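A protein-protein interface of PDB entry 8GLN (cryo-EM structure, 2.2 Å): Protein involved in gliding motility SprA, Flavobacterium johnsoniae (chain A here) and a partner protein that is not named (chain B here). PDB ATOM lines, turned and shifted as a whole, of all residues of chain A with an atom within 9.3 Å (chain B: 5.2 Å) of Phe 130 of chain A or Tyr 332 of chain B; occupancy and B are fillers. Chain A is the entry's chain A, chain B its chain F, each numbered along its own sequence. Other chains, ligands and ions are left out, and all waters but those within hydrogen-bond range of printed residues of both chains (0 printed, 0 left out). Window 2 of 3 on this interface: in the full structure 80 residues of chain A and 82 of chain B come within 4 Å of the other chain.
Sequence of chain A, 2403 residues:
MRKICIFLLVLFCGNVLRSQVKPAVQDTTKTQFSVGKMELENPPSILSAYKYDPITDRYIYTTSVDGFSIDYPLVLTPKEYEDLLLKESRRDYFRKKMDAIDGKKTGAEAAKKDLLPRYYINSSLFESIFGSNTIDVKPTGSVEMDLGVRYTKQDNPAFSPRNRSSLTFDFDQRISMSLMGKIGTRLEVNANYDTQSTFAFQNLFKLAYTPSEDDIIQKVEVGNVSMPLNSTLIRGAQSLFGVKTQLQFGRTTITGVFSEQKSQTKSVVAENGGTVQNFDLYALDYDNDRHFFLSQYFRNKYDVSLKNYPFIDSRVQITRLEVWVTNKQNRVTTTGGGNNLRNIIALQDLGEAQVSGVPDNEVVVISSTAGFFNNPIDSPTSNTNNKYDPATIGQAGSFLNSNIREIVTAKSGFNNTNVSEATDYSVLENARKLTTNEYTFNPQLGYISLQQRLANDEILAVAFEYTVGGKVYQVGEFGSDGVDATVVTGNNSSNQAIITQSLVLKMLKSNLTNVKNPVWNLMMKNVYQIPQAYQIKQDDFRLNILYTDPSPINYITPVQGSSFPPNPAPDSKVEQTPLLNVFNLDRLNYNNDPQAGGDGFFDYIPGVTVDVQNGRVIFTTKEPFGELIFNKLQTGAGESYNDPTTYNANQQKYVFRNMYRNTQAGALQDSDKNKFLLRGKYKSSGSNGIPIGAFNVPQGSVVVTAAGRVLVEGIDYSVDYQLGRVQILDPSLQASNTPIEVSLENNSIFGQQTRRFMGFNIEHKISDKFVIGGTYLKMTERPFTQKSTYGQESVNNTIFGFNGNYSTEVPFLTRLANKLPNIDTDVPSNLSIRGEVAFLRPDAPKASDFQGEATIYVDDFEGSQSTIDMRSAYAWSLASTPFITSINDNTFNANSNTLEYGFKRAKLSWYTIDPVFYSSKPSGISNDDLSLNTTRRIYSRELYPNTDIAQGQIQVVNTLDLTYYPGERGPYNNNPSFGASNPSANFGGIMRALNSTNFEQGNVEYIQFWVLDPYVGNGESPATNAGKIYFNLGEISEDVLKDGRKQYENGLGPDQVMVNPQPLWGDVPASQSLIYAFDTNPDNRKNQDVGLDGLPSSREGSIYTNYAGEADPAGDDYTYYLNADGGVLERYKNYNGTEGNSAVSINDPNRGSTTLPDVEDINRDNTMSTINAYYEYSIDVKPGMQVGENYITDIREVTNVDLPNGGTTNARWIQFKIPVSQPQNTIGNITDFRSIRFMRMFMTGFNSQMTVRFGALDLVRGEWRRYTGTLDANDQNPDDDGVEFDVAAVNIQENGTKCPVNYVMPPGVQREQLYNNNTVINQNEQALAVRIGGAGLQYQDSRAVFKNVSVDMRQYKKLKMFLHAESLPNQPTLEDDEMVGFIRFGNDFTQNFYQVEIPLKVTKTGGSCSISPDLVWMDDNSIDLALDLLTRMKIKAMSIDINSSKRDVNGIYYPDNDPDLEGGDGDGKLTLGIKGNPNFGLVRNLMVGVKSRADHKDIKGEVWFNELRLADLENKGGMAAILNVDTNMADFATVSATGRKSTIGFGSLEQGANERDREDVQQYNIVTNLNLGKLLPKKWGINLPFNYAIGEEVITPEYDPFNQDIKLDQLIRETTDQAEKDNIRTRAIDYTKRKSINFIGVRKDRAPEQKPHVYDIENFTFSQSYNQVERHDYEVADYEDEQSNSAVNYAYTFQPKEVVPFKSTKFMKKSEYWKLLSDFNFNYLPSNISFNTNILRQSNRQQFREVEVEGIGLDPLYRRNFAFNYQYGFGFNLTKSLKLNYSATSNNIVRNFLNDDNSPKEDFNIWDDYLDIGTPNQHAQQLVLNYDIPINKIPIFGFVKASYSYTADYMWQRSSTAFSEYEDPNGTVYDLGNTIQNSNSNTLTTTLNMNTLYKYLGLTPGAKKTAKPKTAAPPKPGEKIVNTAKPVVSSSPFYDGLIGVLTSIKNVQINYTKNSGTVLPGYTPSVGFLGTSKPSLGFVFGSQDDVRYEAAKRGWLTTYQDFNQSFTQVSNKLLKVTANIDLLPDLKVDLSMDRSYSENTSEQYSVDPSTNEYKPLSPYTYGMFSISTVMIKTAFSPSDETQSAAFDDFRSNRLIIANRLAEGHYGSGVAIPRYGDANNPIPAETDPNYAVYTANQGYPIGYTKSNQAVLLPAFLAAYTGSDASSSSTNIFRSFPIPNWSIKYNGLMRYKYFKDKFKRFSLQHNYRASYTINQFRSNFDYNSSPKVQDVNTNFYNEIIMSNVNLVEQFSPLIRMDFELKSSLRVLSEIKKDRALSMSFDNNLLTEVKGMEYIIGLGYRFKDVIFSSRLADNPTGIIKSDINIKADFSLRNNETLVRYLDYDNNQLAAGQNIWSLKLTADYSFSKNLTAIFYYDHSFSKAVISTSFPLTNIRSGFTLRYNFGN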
ATOM      1  N   ILE A 129     -17.846  15.509 -13.567  1.00  0.00           N
ATOM      2  CA  ILE A 129     -16.850  14.760 -12.813  1.00  0.00           C
ATOM      3  C   ILE A 129     -15.488  14.898 -13.489  1.00  0.00           C
ATOM      4  O   ILE A 129     -14.448  14.850 -12.833  1.00  0.00           O
ATOM      5  CB  ILE A 129     -17.268  13.281 -12.657  1.00  0.00           C
ATOM      6  CG1 ILE A 129     -16.310  12.542 -11.722  1.00  0.00           C
ATOM      7  CG2 ILE A 129     -17.357  12.594 -14.014  1.00  0.00           C
ATOM      8  CD1 ILE A 129     -16.845  11.215 -11.234  1.00  0.00           C
ATOM      9  N   PHE A 130     -15.505  15.086 -14.805  1.00  0.00           N
ATOM     10  CA  PHE A 130     -14.313  15.364 -15.587  1.00  0.00           C
ATOM     11  C   PHE A 130     -14.527  16.639 -16.395  1.00  0.00           C
ATOM     12  O   PHE A 130     -15.661  17.064 -16.634  1.00  0.00           O
ATOM     13  CB  PHE A 130     -13.959  14.194 -16.514  1.00  0.00           C
ATOM     14  CG  PHE A 130     -13.754  12.890 -15.794  1.00  0.00           C
ATOM     15  CD1 PHE A 130     -12.921  12.817 -14.690  1.00  0.00           C
ATOM     16  CD2 PHE A 130     -14.393  11.738 -16.221  1.00  0.00           C
ATOM     17  CE1 PHE A 130     -12.731  11.620 -14.024  1.00  0.00           C
ATOM     18  CE2 PHE A 130     -14.207  10.538 -15.559  1.00  0.00           C
ATOM     19  CZ  PHE A 130     -13.376  10.480 -14.459  1.00  0.00           C
ATOM     20  N   GLY A 131     -13.415  17.250 -16.807  1.00  0.00           N
ATOM     21  CA  GLY A 131     -13.494  18.548 -17.455  1.00  0.00           C
ATOM     22  C   GLY A 131     -14.238  18.516 -18.777  1.00  0.00           C
ATOM     23  O   GLY A 131     -15.017  19.422 -19.083  1.00  0.00           O
ATOM     24  N   SER A 132     -14.012  17.478 -19.577  1.00  0.00           N
ATOM     25  CA  SER A 132     -14.644  17.365 -20.886  1.00  0.00           C
ATOM     26  C   SER A 132     -15.023  15.906 -21.114  1.00  0.00           C
ATOM     27  O   SER A 132     -14.974  15.077 -20.200  1.00  0.00           O
ATOM     28  CB  SER A 132     -13.719  17.906 -21.984  1.00  0.00           C
ATOM     29  OG  SER A 132     -12.565  17.099 -22.127  1.00  0.00           O
ATOM     30  N   ASN A 133     -15.413  15.593 -22.350  1.00  0.00           N
ATOM     31  CA  ASN A 133     -15.825  14.249 -22.726  1.00  0.00           C
ATOM     32  C   ASN A 133     -14.807  13.536 -23.605  1.00  0.00           C
ATOM     33  O   ASN A 133     -15.057  12.399 -24.016  1.00  0.00           O
ATOM     34  CB  ASN A 133     -17.178  14.296 -23.447  1.00  0.00           C
ATOM     35  CG  ASN A 133     -18.350  14.316 -22.488  1.00  0.00           C
ATOM     36  OD1 ASN A 133     -18.751  13.280 -21.956  1.00  0.00           O
ATOM     37  ND2 ASN A 133     -18.909  15.499 -22.261  1.00  0.00           N
ATOM     38  N   THR A 134     -13.675  14.167 -23.905  1.00  0.00           N
ATOM     39  CA  THR A 134     -12.686  13.561 -24.783  1.00  0.00           C
ATOM     40  C   THR A 134     -11.931  12.449 -24.064  1.00  0.00           C
ATOM     41  O   THR A 134     -11.714  12.506 -22.849  1.00  0.00           O
ATOM     42  CB  THR A 134     -11.705  14.616 -25.302  1.00  0.00           C
ATOM     43  OG1 THR A 134     -10.834  14.026 -26.275  1.00  0.00           O
ATOM     44  CG2 THR A 134     -10.875  15.197 -24.166  1.00  0.00           C
ATOM     45  N   ILE A 135     -11.556  11.423 -24.822  1.00  0.00           N
ATOM     46  CA  ILE A 135     -10.766  10.301 -24.326  1.00  0.00           C
ATOM     47  C   ILE A 135      -9.710  10.003 -25.381  1.00  0.00           C
ATOM     48  O   ILE A 135     -10.033   9.481 -26.456  1.00  0.00           O
ATOM     49  CB  ILE A 135     -11.623   9.060 -24.040  1.00  0.00           C
ATOM     50  CG1 ILE A 135     -12.633   9.352 -22.926  1.00  0.00           C
ATOM     51  CG2 ILE A 135     -10.741   7.879 -23.665  1.00  0.00           C
ATOM     52  CD1 ILE A 135     -13.678   8.278 -22.745  1.00  0.00           C
ATOM     53  N   ASP A 136      -8.457  10.330 -25.083  1.00  0.00           N
ATOM     54  CA  ASP A 136      -7.367  10.224 -26.045  1.00  0.00           C
ATOM     55  C   ASP A 136      -6.204   9.430 -25.467  1.00  0.00           C
ATOM     56  O   ASP A 136      -5.040   9.829 -25.570  1.00  0.00           O
ATOM     57  CB  ASP A 136      -6.908  11.607 -26.502  1.00  0.00           C
ATOM     58  CG  ASP A 136      -6.482  12.492 -25.348  1.00  0.00           C
ATOM     59  OD1 ASP A 136      -5.262  12.631 -25.119  1.00  0.00           O
ATOM     60  OD2 ASP A 136      -7.369  13.051 -24.669  1.00  0.00           O
ATOM     61  N   LYS A 182      -5.248  11.217 -21.834  1.00  0.00           N
ATOM     62  CA  LYS A 182      -6.068  11.929 -20.867  1.00  0.00           C
ATOM     63  C   LYS A 182      -7.530  11.563 -21.073  1.00  0.00           C
ATOM     64  O   LYS A 182      -7.940  11.175 -22.169  1.00  0.00           O
ATOM     65  CB  LYS A 182      -5.890  13.449 -20.990  1.00  0.00           C
ATOM     66  CG  LYS A 182      -4.515  13.955 -20.589  1.00  0.00           C
ATOM     67  CD  LYS A 182      -4.361  15.437 -20.879  1.00  0.00           C
ATOM     68  CE  LYS A 182      -5.228  16.274 -19.955  1.00  0.00           C
ATOM     69  NZ  LYS A 182      -4.768  16.198 -18.542  1.00  0.00           N
ATOM     70  N   ILE A 183      -8.314  11.689 -20.005  1.00  0.00           N
ATOM     71  CA  ILE A 183      -9.760  11.494 -20.051  1.00  0.00           C
ATOM     72  C   ILE A 183     -10.412  12.770 -19.535  1.00  0.00           C
ATOM     73  O   ILE A 183     -10.421  13.024 -18.323  1.00  0.00           O
ATOM     74  CB  ILE A 183     -10.216  10.277 -19.234  1.00  0.00           C
ATOM     75  CG1 ILE A 183      -9.699   8.979 -19.851  1.00  0.00           C
ATOM     76  CG2 ILE A 183     -11.733  10.233 -19.140  1.00  0.00           C
ATOM     77  CD1 ILE A 183      -8.423   8.488 -19.238  1.00  0.00           C
ATOM     78  N   GLY A 184     -10.954  13.569 -20.448  1.00  0.00           N
ATOM     79  CA  GLY A 184     -11.687  14.766 -20.063  1.00  0.00           C
ATOM     80  C   GLY A 184     -10.864  15.804 -19.334  1.00  0.00           C
ATOM     81  O   GLY A 184     -11.331  16.369 -18.338  1.00  0.00           O
ATOM     82  N   THR A 185      -9.621  16.021 -19.774  1.00  0.00           N
ATOM     83  CA  THR A 185      -8.718  17.084 -19.324  1.00  0.00           C
ATOM     84  C   THR A 185      -8.571  17.149 -17.804  1.00  0.00           C
ATOM     85  O   THR A 185      -8.038  18.126 -17.268  1.00  0.00           O
ATOM     86  CB  THR A 185      -9.147  18.453 -19.887  1.00  0.00           C
ATOM     87  OG1 THR A 185      -8.039  19.358 -19.821  1.00  0.00           O
ATOM     88  CG2 THR A 185     -10.312  19.066 -19.113  1.00  0.00           C
ATOM     89  N   ARG A 186      -9.002  16.103 -17.105  1.00  0.00           N
ATOM     90  CA  ARG A 186      -8.864  16.011 -15.659  1.00  0.00           C
ATOM     91  C   ARG A 186      -8.176  14.739 -15.195  1.00  0.00           C
ATOM     92  O   ARG A 186      -7.489  14.765 -14.172  1.00  0.00           O
ATOM     93  CB  ARG A 186     -10.238  16.102 -14.979  1.00  0.00           C
ATOM     94  CG  ARG A 186     -10.664  17.515 -14.625  1.00  0.00           C
ATOM     95  CD  ARG A 186     -11.578  17.516 -13.407  1.00  0.00           C
ATOM     96  NE  ARG A 186     -12.771  18.342 -13.569  1.00  0.00           N
ATOM     97  CZ  ARG A 186     -12.772  19.648 -13.813  1.00  0.00           C
ATOM     98  NH1 ARG A 186     -11.649  20.344 -13.883  1.00  0.00           N
ATOM     99  NH2 ARG A 186     -13.935  20.275 -13.972  1.00  0.00           N
ATOM    100  N   LEU A 187      -8.339  13.634 -15.914  1.00  0.00           N
ATOM    101  CA  LEU A 187      -7.696  12.372 -15.584  1.00  0.00           C
ATOM    102  C   LEU A 187      -6.557  12.119 -16.562  1.00  0.00           C
ATOM    103  O   LEU A 187      -6.757  12.170 -17.778  1.00  0.00           O
ATOM    104  CB  LEU A 187      -8.704  11.224 -15.632  1.00  0.00           C
ATOM    105  CG  LEU A 187      -8.292   9.887 -15.020  1.00  0.00           C
ATOM    106  CD1 LEU A 187      -7.658  10.082 -13.656  1.00  0.00           C
ATOM    107  CD2 LEU A 187      -9.502   8.987 -14.914  1.00  0.00           C
ATOM    108  N   GLU A 188      -5.370  11.852 -16.031  1.00  0.00           N
ATOM    109  CA  GLU A 188      -4.184  11.608 -16.837  1.00  0.00           C
ATOM    110  C   GLU A 188      -3.707  10.178 -16.624  1.00  0.00           C
ATOM    111  O   GLU A 188      -3.710   9.675 -15.497  1.00  0.00           O
ATOM    112  CB  GLU A 188      -3.071  12.601 -16.487  1.00  0.00           C
ATOM    113  CG  GLU A 188      -1.718  12.269 -17.089  1.00  0.00           C
ATOM    114  CD  GLU A 188      -0.840  13.493 -17.260  1.00  0.00           C
ATOM    115  OE1 GLU A 188       0.288  13.349 -17.778  1.00  0.00           O
ATOM    116  OE2 GLU A 188      -1.275  14.599 -16.877  1.00  0.00           O
ATOM    117  N   LEU A 207      -2.492   6.799 -12.507  1.00  0.00           N
ATOM    118  CA  LEU A 207      -3.752   7.483 -12.765  1.00  0.00           C
ATOM    119  C   LEU A 207      -3.794   8.733 -11.899  1.00  0.00           C
ATOM    120  O   LEU A 207      -3.723   8.639 -10.669  1.00  0.00           O
ATOM    121  CB  LEU A 207      -4.943   6.576 -12.459  1.00  0.00           C
ATOM    122  CG  LEU A 207      -5.547   5.794 -13.624  1.00  0.00           C
ATOM    123  CD1 LEU A 207      -6.719   4.956 -13.146  1.00  0.00           C
ATOM    124  CD2 LEU A 207      -5.984   6.745 -14.719  1.00  0.00           C
ATOM    125  N   ALA A 208      -3.913   9.898 -12.532  1.00  0.00           N
ATOM    126  CA  ALA A 208      -3.862  11.179 -11.836  1.00  0.00           C
ATOM    127  C   ALA A 208      -5.124  11.968 -12.153  1.00  0.00           C
ATOM    128  O   ALA A 208      -5.350  12.348 -13.306  1.00  0.00           O
ATOM    129  CB  ALA A 208      -2.612  11.964 -12.227  1.00  0.00           C
ATOM    130  N   TYR A 209      -5.935  12.223 -11.130  1.00  0.00           N
ATOM    131  CA  TYR A 209      -7.168  12.989 -11.267  1.00  0.00           C
ATOM    132  C   TYR A 209      -6.959  14.356 -10.628  1.00  0.00           C
ATOM    133  O   TYR A 209      -6.908  14.474  -9.400  1.00  0.00           O
ATOM    134  CB  TYR A 209      -8.338  12.253 -10.619  1.00  0.00           C
ATOM    135  CG  TYR A 209      -9.586  13.092 -10.478  1.00  0.00           C
ATOM    136  CD1 TYR A 209     -10.225  13.612 -11.595  1.00  0.00           C
ATOM    137  CD2 TYR A 209     -10.123  13.368  -9.229  1.00  0.00           C
ATOM    138  CE1 TYR A 209     -11.365  14.380 -11.471  1.00  0.00           C
ATOM    139  CE2 TYR A 209     -11.262  14.136  -9.095  1.00  0.00           C
ATOM    140  CZ  TYR A 209     -11.879  14.639 -10.219  1.00  0.00           C
ATOM    141  OH  TYR A 209     -13.014  15.405 -10.092  1.00  0.00           O
ATOM    142  N   THR A 210      -6.843  15.389 -11.461  1.00  0.00           N
ATOM    143  CA  THR A 210      -6.600  16.746 -10.982  1.00  0.00           C
ATOM    144  C   THR A 210      -7.826  17.610 -11.245  1.00  0.00           C
ATOM    145  O   THR A 210      -8.034  18.066 -12.380  1.00  0.00           O
ATOM    146  CB  THR A 210      -5.367  17.347 -11.662  1.00  0.00           C
ATOM    147  OG1 THR A 210      -4.217  16.547 -11.362  1.00  0.00           O
ATOM    148  CG2 THR A 210      -5.126  18.765 -11.171  1.00  0.00           C
ATOM    149  N   PRO A 211      -8.668  17.860 -10.243  1.00  0.00           N
ATOM    150  CA  PRO A 211      -9.826  18.738 -10.451  1.00  0.00           C
ATOM    151  C   PRO A 211      -9.475  20.208 -10.290  1.00  0.00           C
ATOM    152  O   PRO A 211      -8.301  20.561 -10.137  1.00  0.00           O
ATOM    153  CB  PRO A 211     -10.822  18.272  -9.380  1.00  0.00           C
ATOM    154  CG  PRO A 211     -10.014  17.493  -8.374  1.00  0.00           C
ATOM    155  CD  PRO A 211      -8.606  17.333  -8.872  1.00  0.00           C
ATOM    156  N   SER A 212     -10.486  21.072 -10.332  1.00  0.00           N
ATOM    157  CA  SER A 212     -10.269  22.503 -10.200  1.00  0.00           C
ATOM    158  C   SER A 212      -9.784  22.848  -8.791  1.00  0.00           C
ATOM    159  O   SER A 212      -9.812  22.026  -7.869  1.00  0.00           O
ATOM    160  CB  SER A 212     -11.549  23.270 -10.528  1.00  0.00           C
ATOM    161  OG  SER A 212     -12.479  23.189  -9.463  1.00  0.00           O
ATOM    162  N   VAL A 220      -5.968  13.167  -6.766  1.00  0.00           N
ATOM    163  CA  VAL A 220      -6.087  11.756  -6.421  1.00  0.00           C
ATOM    164  C   VAL A 220      -5.200  10.966  -7.369  1.00  0.00           C
ATOM    165  O   VAL A 220      -5.288  11.129  -8.591  1.00  0.00           O
ATOM    166  CB  VAL A 220      -7.545  11.267  -6.499  1.00  0.00           C
ATOM    167  CG1 VAL A 220      -7.606   9.756  -6.346  1.00  0.00           C
ATOM    168  CG2 VAL A 220      -8.384  11.940  -5.432  1.00  0.00           C
ATOM    169  N   TYR B 244     -24.469   8.069 -20.217  1.00  0.00           N
ATOM    170  CA  TYR B 244     -23.042   7.969 -20.485  1.00  0.00           C
ATOM    171  C   TYR B 244     -22.229   7.514 -19.285  1.00  0.00           C
ATOM    172  O   TYR B 244     -21.088   7.078 -19.469  1.00  0.00           O
ATOM    173  CB  TYR B 244     -22.487   9.317 -20.971  1.00  0.00           C
ATOM    174  CG  TYR B 244     -22.542   9.512 -22.470  1.00  0.00           C
ATOM    175  CD1 TYR B 244     -22.825   8.451 -23.319  1.00  0.00           C
ATOM    176  CD2 TYR B 244     -22.307  10.759 -23.035  1.00  0.00           C
ATOM    177  CE1 TYR B 244     -22.875   8.626 -24.688  1.00  0.00           C
ATOM    178  CE2 TYR B 244     -22.355  10.943 -24.403  1.00  0.00           C
ATOM    179  CZ  TYR B 244     -22.640   9.874 -25.225  1.00  0.00           C
ATOM    180  OH  TYR B 244     -22.688  10.052 -26.589  1.00  0.00           O
ATOM    181  N   ASN B 245     -22.770   7.601 -18.073  1.00  0.00           N
ATOM    182  CA  ASN B 245     -22.095   7.143 -16.868  1.00  0.00           C
ATOM    183  C   ASN B 245     -22.827   5.916 -16.347  1.00  0.00           C
ATOM    184  O   ASN B 245     -24.036   5.967 -16.104  1.00  0.00           O
ATOM    185  CB  ASN B 245     -22.061   8.238 -15.800  1.00  0.00           C
ATOM    186  CG  ASN B 245     -20.989   9.279 -16.063  1.00  0.00           C
ATOM    187  OD1 ASN B 245     -20.506   9.936 -15.141  1.00  0.00           O
ATOM    188  ND2 ASN B 245     -20.612   9.435 -17.327  1.00  0.00           N
ATOM    189  N   TYR B 330     -17.410   1.204 -12.567  1.00  0.00           N
ATOM    190  CA  TYR B 330     -17.892   2.472 -13.096  1.00  0.00           C
ATOM    191  C   TYR B 330     -17.363   2.664 -14.512  1.00  0.00           C
ATOM    192  O   TYR B 330     -16.162   2.512 -14.755  1.00  0.00           O
ATOM    193  CB  TYR B 330     -17.459   3.639 -12.209  1.00  0.00           C
ATOM    194  CG  TYR B 330     -17.683   4.993 -12.843  1.00  0.00           C
ATOM    195  CD1 TYR B 330     -18.966   5.474 -13.062  1.00  0.00           C
ATOM    196  CD2 TYR B 330     -16.611   5.785 -13.230  1.00  0.00           C
ATOM    197  CE1 TYR B 330     -19.177   6.707 -13.646  1.00  0.00           C
ATOM    198  CE2 TYR B 330     -16.812   7.020 -13.814  1.00  0.00           C
ATOM    199  CZ  TYR B 330     -18.096   7.477 -14.019  1.00  0.00           C
ATOM    200  OH  TYR B 330     -18.300   8.707 -14.600  1.00  0.00           O
ATOM    201  N   MET B 331     -18.256   3.002 -15.436  1.00  0.00           N
ATOM    202  CA  MET B 331     -17.916   3.164 -16.843  1.00  0.00           C
ATOM    203  C   MET B 331     -18.163   4.601 -17.278  1.00  0.00           C
ATOM    204  O   MET B 331     -19.237   5.156 -17.022  1.00  0.00           O
ATOM    205  CB  MET B 331     -18.727   2.203 -17.714  1.00  0.00           C
ATOM    206  CG  MET B 331     -18.050   0.866 -17.958  1.00  0.00           C
ATOM    207  SD  MET B 331     -16.758   0.961 -19.210  1.00  0.00           S
ATOM    208  CE  MET B 331     -17.369  -0.210 -20.417  1.00  0.00           C
ATOM    209  N   TYR B 332     -17.171   5.197 -17.935  1.00  0.00           N
ATOM    210  CA  TYR B 332     -17.266   6.548 -18.473  1.00  0.00           C
ATOM    211  C   TYR B 332     -17.172   6.478 -19.989  1.00  0.00           C
ATOM    212  O   TYR B 332     -16.135   6.079 -20.531  1.00  0.00           O
ATOM    213  CB  TYR B 332     -16.162   7.445 -17.909  1.00  0.00           C
ATOM    214  CG  TYR B 332     -16.283   8.894 -18.321  1.00  0.00           C
ATOM    215  CD1 TYR B 332     -17.426   9.625 -18.033  1.00  0.00           C
ATOM    216  CD2 TYR B 332     -15.254   9.529 -19.006  1.00  0.00           C
ATOM    217  CE1 TYR B 332     -17.541  10.948 -18.409  1.00  0.00           C
ATOM    218  CE2 TYR B 332     -15.362  10.852 -19.387  1.00  0.00           C
ATOM    219  CZ  TYR B 332     -16.507  11.557 -19.086  1.00  0.00           C
ATOM    220  OH  TYR B 332     -16.620  12.875 -19.463  1.00  0.00           O
ATOM    221  N   GLN B 333     -18.256   6.859 -20.669  1.00  0.00           N
ATOM    222  CA  GLN B 333     -18.341   6.878 -22.131  1.00  0.00           C
ATOM    223  C   GLN B 333     -18.079   5.510 -22.753  1.00  0.00           C
ATOM    224  O   GLN B 333     -17.771   5.424 -23.948  1.00  0.00           O
ATOM    225  CB  GLN B 333     -17.389   7.916 -22.738  1.00  0.00           C
ATOM    226  CG  GLN B 333     -17.289   9.218 -21.964  1.00  0.00           C
ATOM    227  CD  GLN B 333     -18.584  10.002 -21.976  1.00  0.00           C
ATOM    228  OE1 GLN B 333     -19.334   9.995 -21.001  1.00  0.00           O
ATOM    229  NE2 GLN B 333     -18.853  10.683 -23.083  1.00  0.00           N
ATOM    230  N   ASP B 334     -18.177   4.440 -21.959  1.00  0.00           N
ATOM    231  CA  ASP B 334     -17.930   3.073 -22.411  1.00  0.00           C
ATOM    232  C   ASP B 334     -16.504   2.889 -22.920  1.00  0.00           C
ATOM    233  O   ASP B 334     -16.191   1.875 -23.550  1.00  0.00           O
ATOM    234  CB  ASP B 334     -18.937   2.670 -23.492  1.00  0.00           C
ATOM    235  CG  ASP B 334     -20.364   2.668 -22.985  1.00  0.00           C
ATOM    236  OD1 ASP B 334     -21.286   2.868 -23.803  1.00  0.00           O
ATOM    237  OD2 ASP B 334     -20.563   2.467 -21.769  1.00  0.00           O
ATOM    238  N   ALA B 335     -15.635   3.866 -22.654  1.00  0.00           N
ATOM    239  CA  ALA B 335     -14.235   3.789 -23.034  1.00  0.00           C
ATOM    240  C   ALA B 335     -13.288   3.880 -21.847  1.00  0.00           C
ATOM    241  O   ALA B 335     -12.088   3.641 -22.014  1.00  0.00           O
ATOM    242  CB  ALA B 335     -13.894   4.896 -24.042  1.00  0.00           C
ATOM    243  N   PHE B 336     -13.790   4.222 -20.665  1.00  0.00           N
ATOM    244  CA  PHE B 336     -13.007   4.220 -19.439  1.00  0.00           C
ATOM    245  C   PHE B 336     -13.774   3.461 -18.368  1.00  0.00           C
ATOM    246  O   PHE B 336     -14.984   3.644 -18.213  1.00  0.00           O
ATOM    247  CB  PHE B 336     -12.707   5.639 -18.951  1.00  0.00           C
ATOM    248  CG  PHE B 336     -11.961   5.679 -17.651  1.00  0.00           C
ATOM    249  CD1 PHE B 336     -10.737   5.046 -17.521  1.00  0.00           C
ATOM    250  CD2 PHE B 336     -12.497   6.324 -16.551  1.00  0.00           C
ATOM    251  CE1 PHE B 336     -10.053   5.072 -16.324  1.00  0.00           C
ATOM    252  CE2 PHE B 336     -11.819   6.351 -15.351  1.00  0.00           C
ATOM    253  CZ  PHE B 336     -10.595   5.724 -15.238  1.00  0.00           C
ATOM    254  N   ALA B 337     -13.066   2.609 -17.631  1.00  0.00           N
ATOM    255  CA  ALA B 337     -13.677   1.794 -16.593  1.00  0.00           C
ATOM    256  C   ALA B 337     -12.831   1.834 -15.332  1.00  0.00           C
ATOM    257  O   ALA B 337     -11.601   1.776 -15.395  1.00  0.00           O
ATOM    258  CB  ALA B 337     -13.855   0.343 -17.055  1.00  0.00           C
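O of Ser 132 of chain A lies within hydrogen-bond range of OH of Tyr 332 of chain B, 2.8 Å away.
OH of Tyr 332 of chain B is in hydrogen-bond range of OD1 of Asn 133 of chain A, 3.3 Å away.
The side-chain amide oxygen of Asn 133 of chain A is in hydrogen-bond range of the side-chain amide nitrogen of Gln 333 of chain B, 2.8 Å away.
N of Ser 132 of chain A sits at hydrogen-bond distance from O of Gly 184 of chain A, at 3.2 Å.
The backbone carbonyl oxygen (O) of Tyr 244 of chain B lies within hydrogen-bond range of the backbone NH (N) of Gln 333 of chain B, 3.1 Å away.
CD2 of Phe 130 of chain A touches CE2 of Tyr 332 of chain B (3.4 Å).
CD1 of Ile 135 of chain A touches O of Tyr 332 of chain B, at 3.97 Å.
Ile 135 of chain A touches Gln 333 of chain B.
Ile 135 of chain A touches Ala 335 of chain B (CD1 to CB, 3.6 Å).
Ile 183 of chain A touches Tyr 332 of chain B.
Leu 187 of chain A touches Phe 336 of chain B (CD2 to CZ, 3.5 Å).
Of chain B, only Tyr 332 comes within 4 Å of Phe 130 of chain A.
Of the printed residues of chain B, Asn 133 of chain A touches Tyr 332 and Gln 333.
Printed residues of chain B within 4 Å of Leu 187 of chain A: Phe 336 (3.5 Å).
Glu 188 of chain A touches none of the printed residues of chain B.
Asn 245 of chain B touches none of the printed residues of chain A.
Of chain A, only Phe 130 (3.4 Å), Ser 132 (2.8 Å), Asn 133 (3.3 Å), Ile 135 (3.97 Å) and Ile 183 (3.6 Å) come within 4 Å of Tyr 332 of chain B.
Gln 333 of chain B touches just these residues of chain A: Asn 133 (2.8 Å) and Ile 135 (3.7 Å).
Printed residues of chain A within 4 Å of Phe 336 of chain B: Leu 187 (3.5 Å).
Hydrophobic or aromatic side chains of chain A that line the printed part of chain B: Phe 130, Ile 135, Ile 183 and Leu 187.
Printed residues of chain B that touch a printed residue of chain A: Tyr 332, Gln 333, Ala 335 and Phe 336.
Among the printed residues, 9 pairs touch across the chains.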
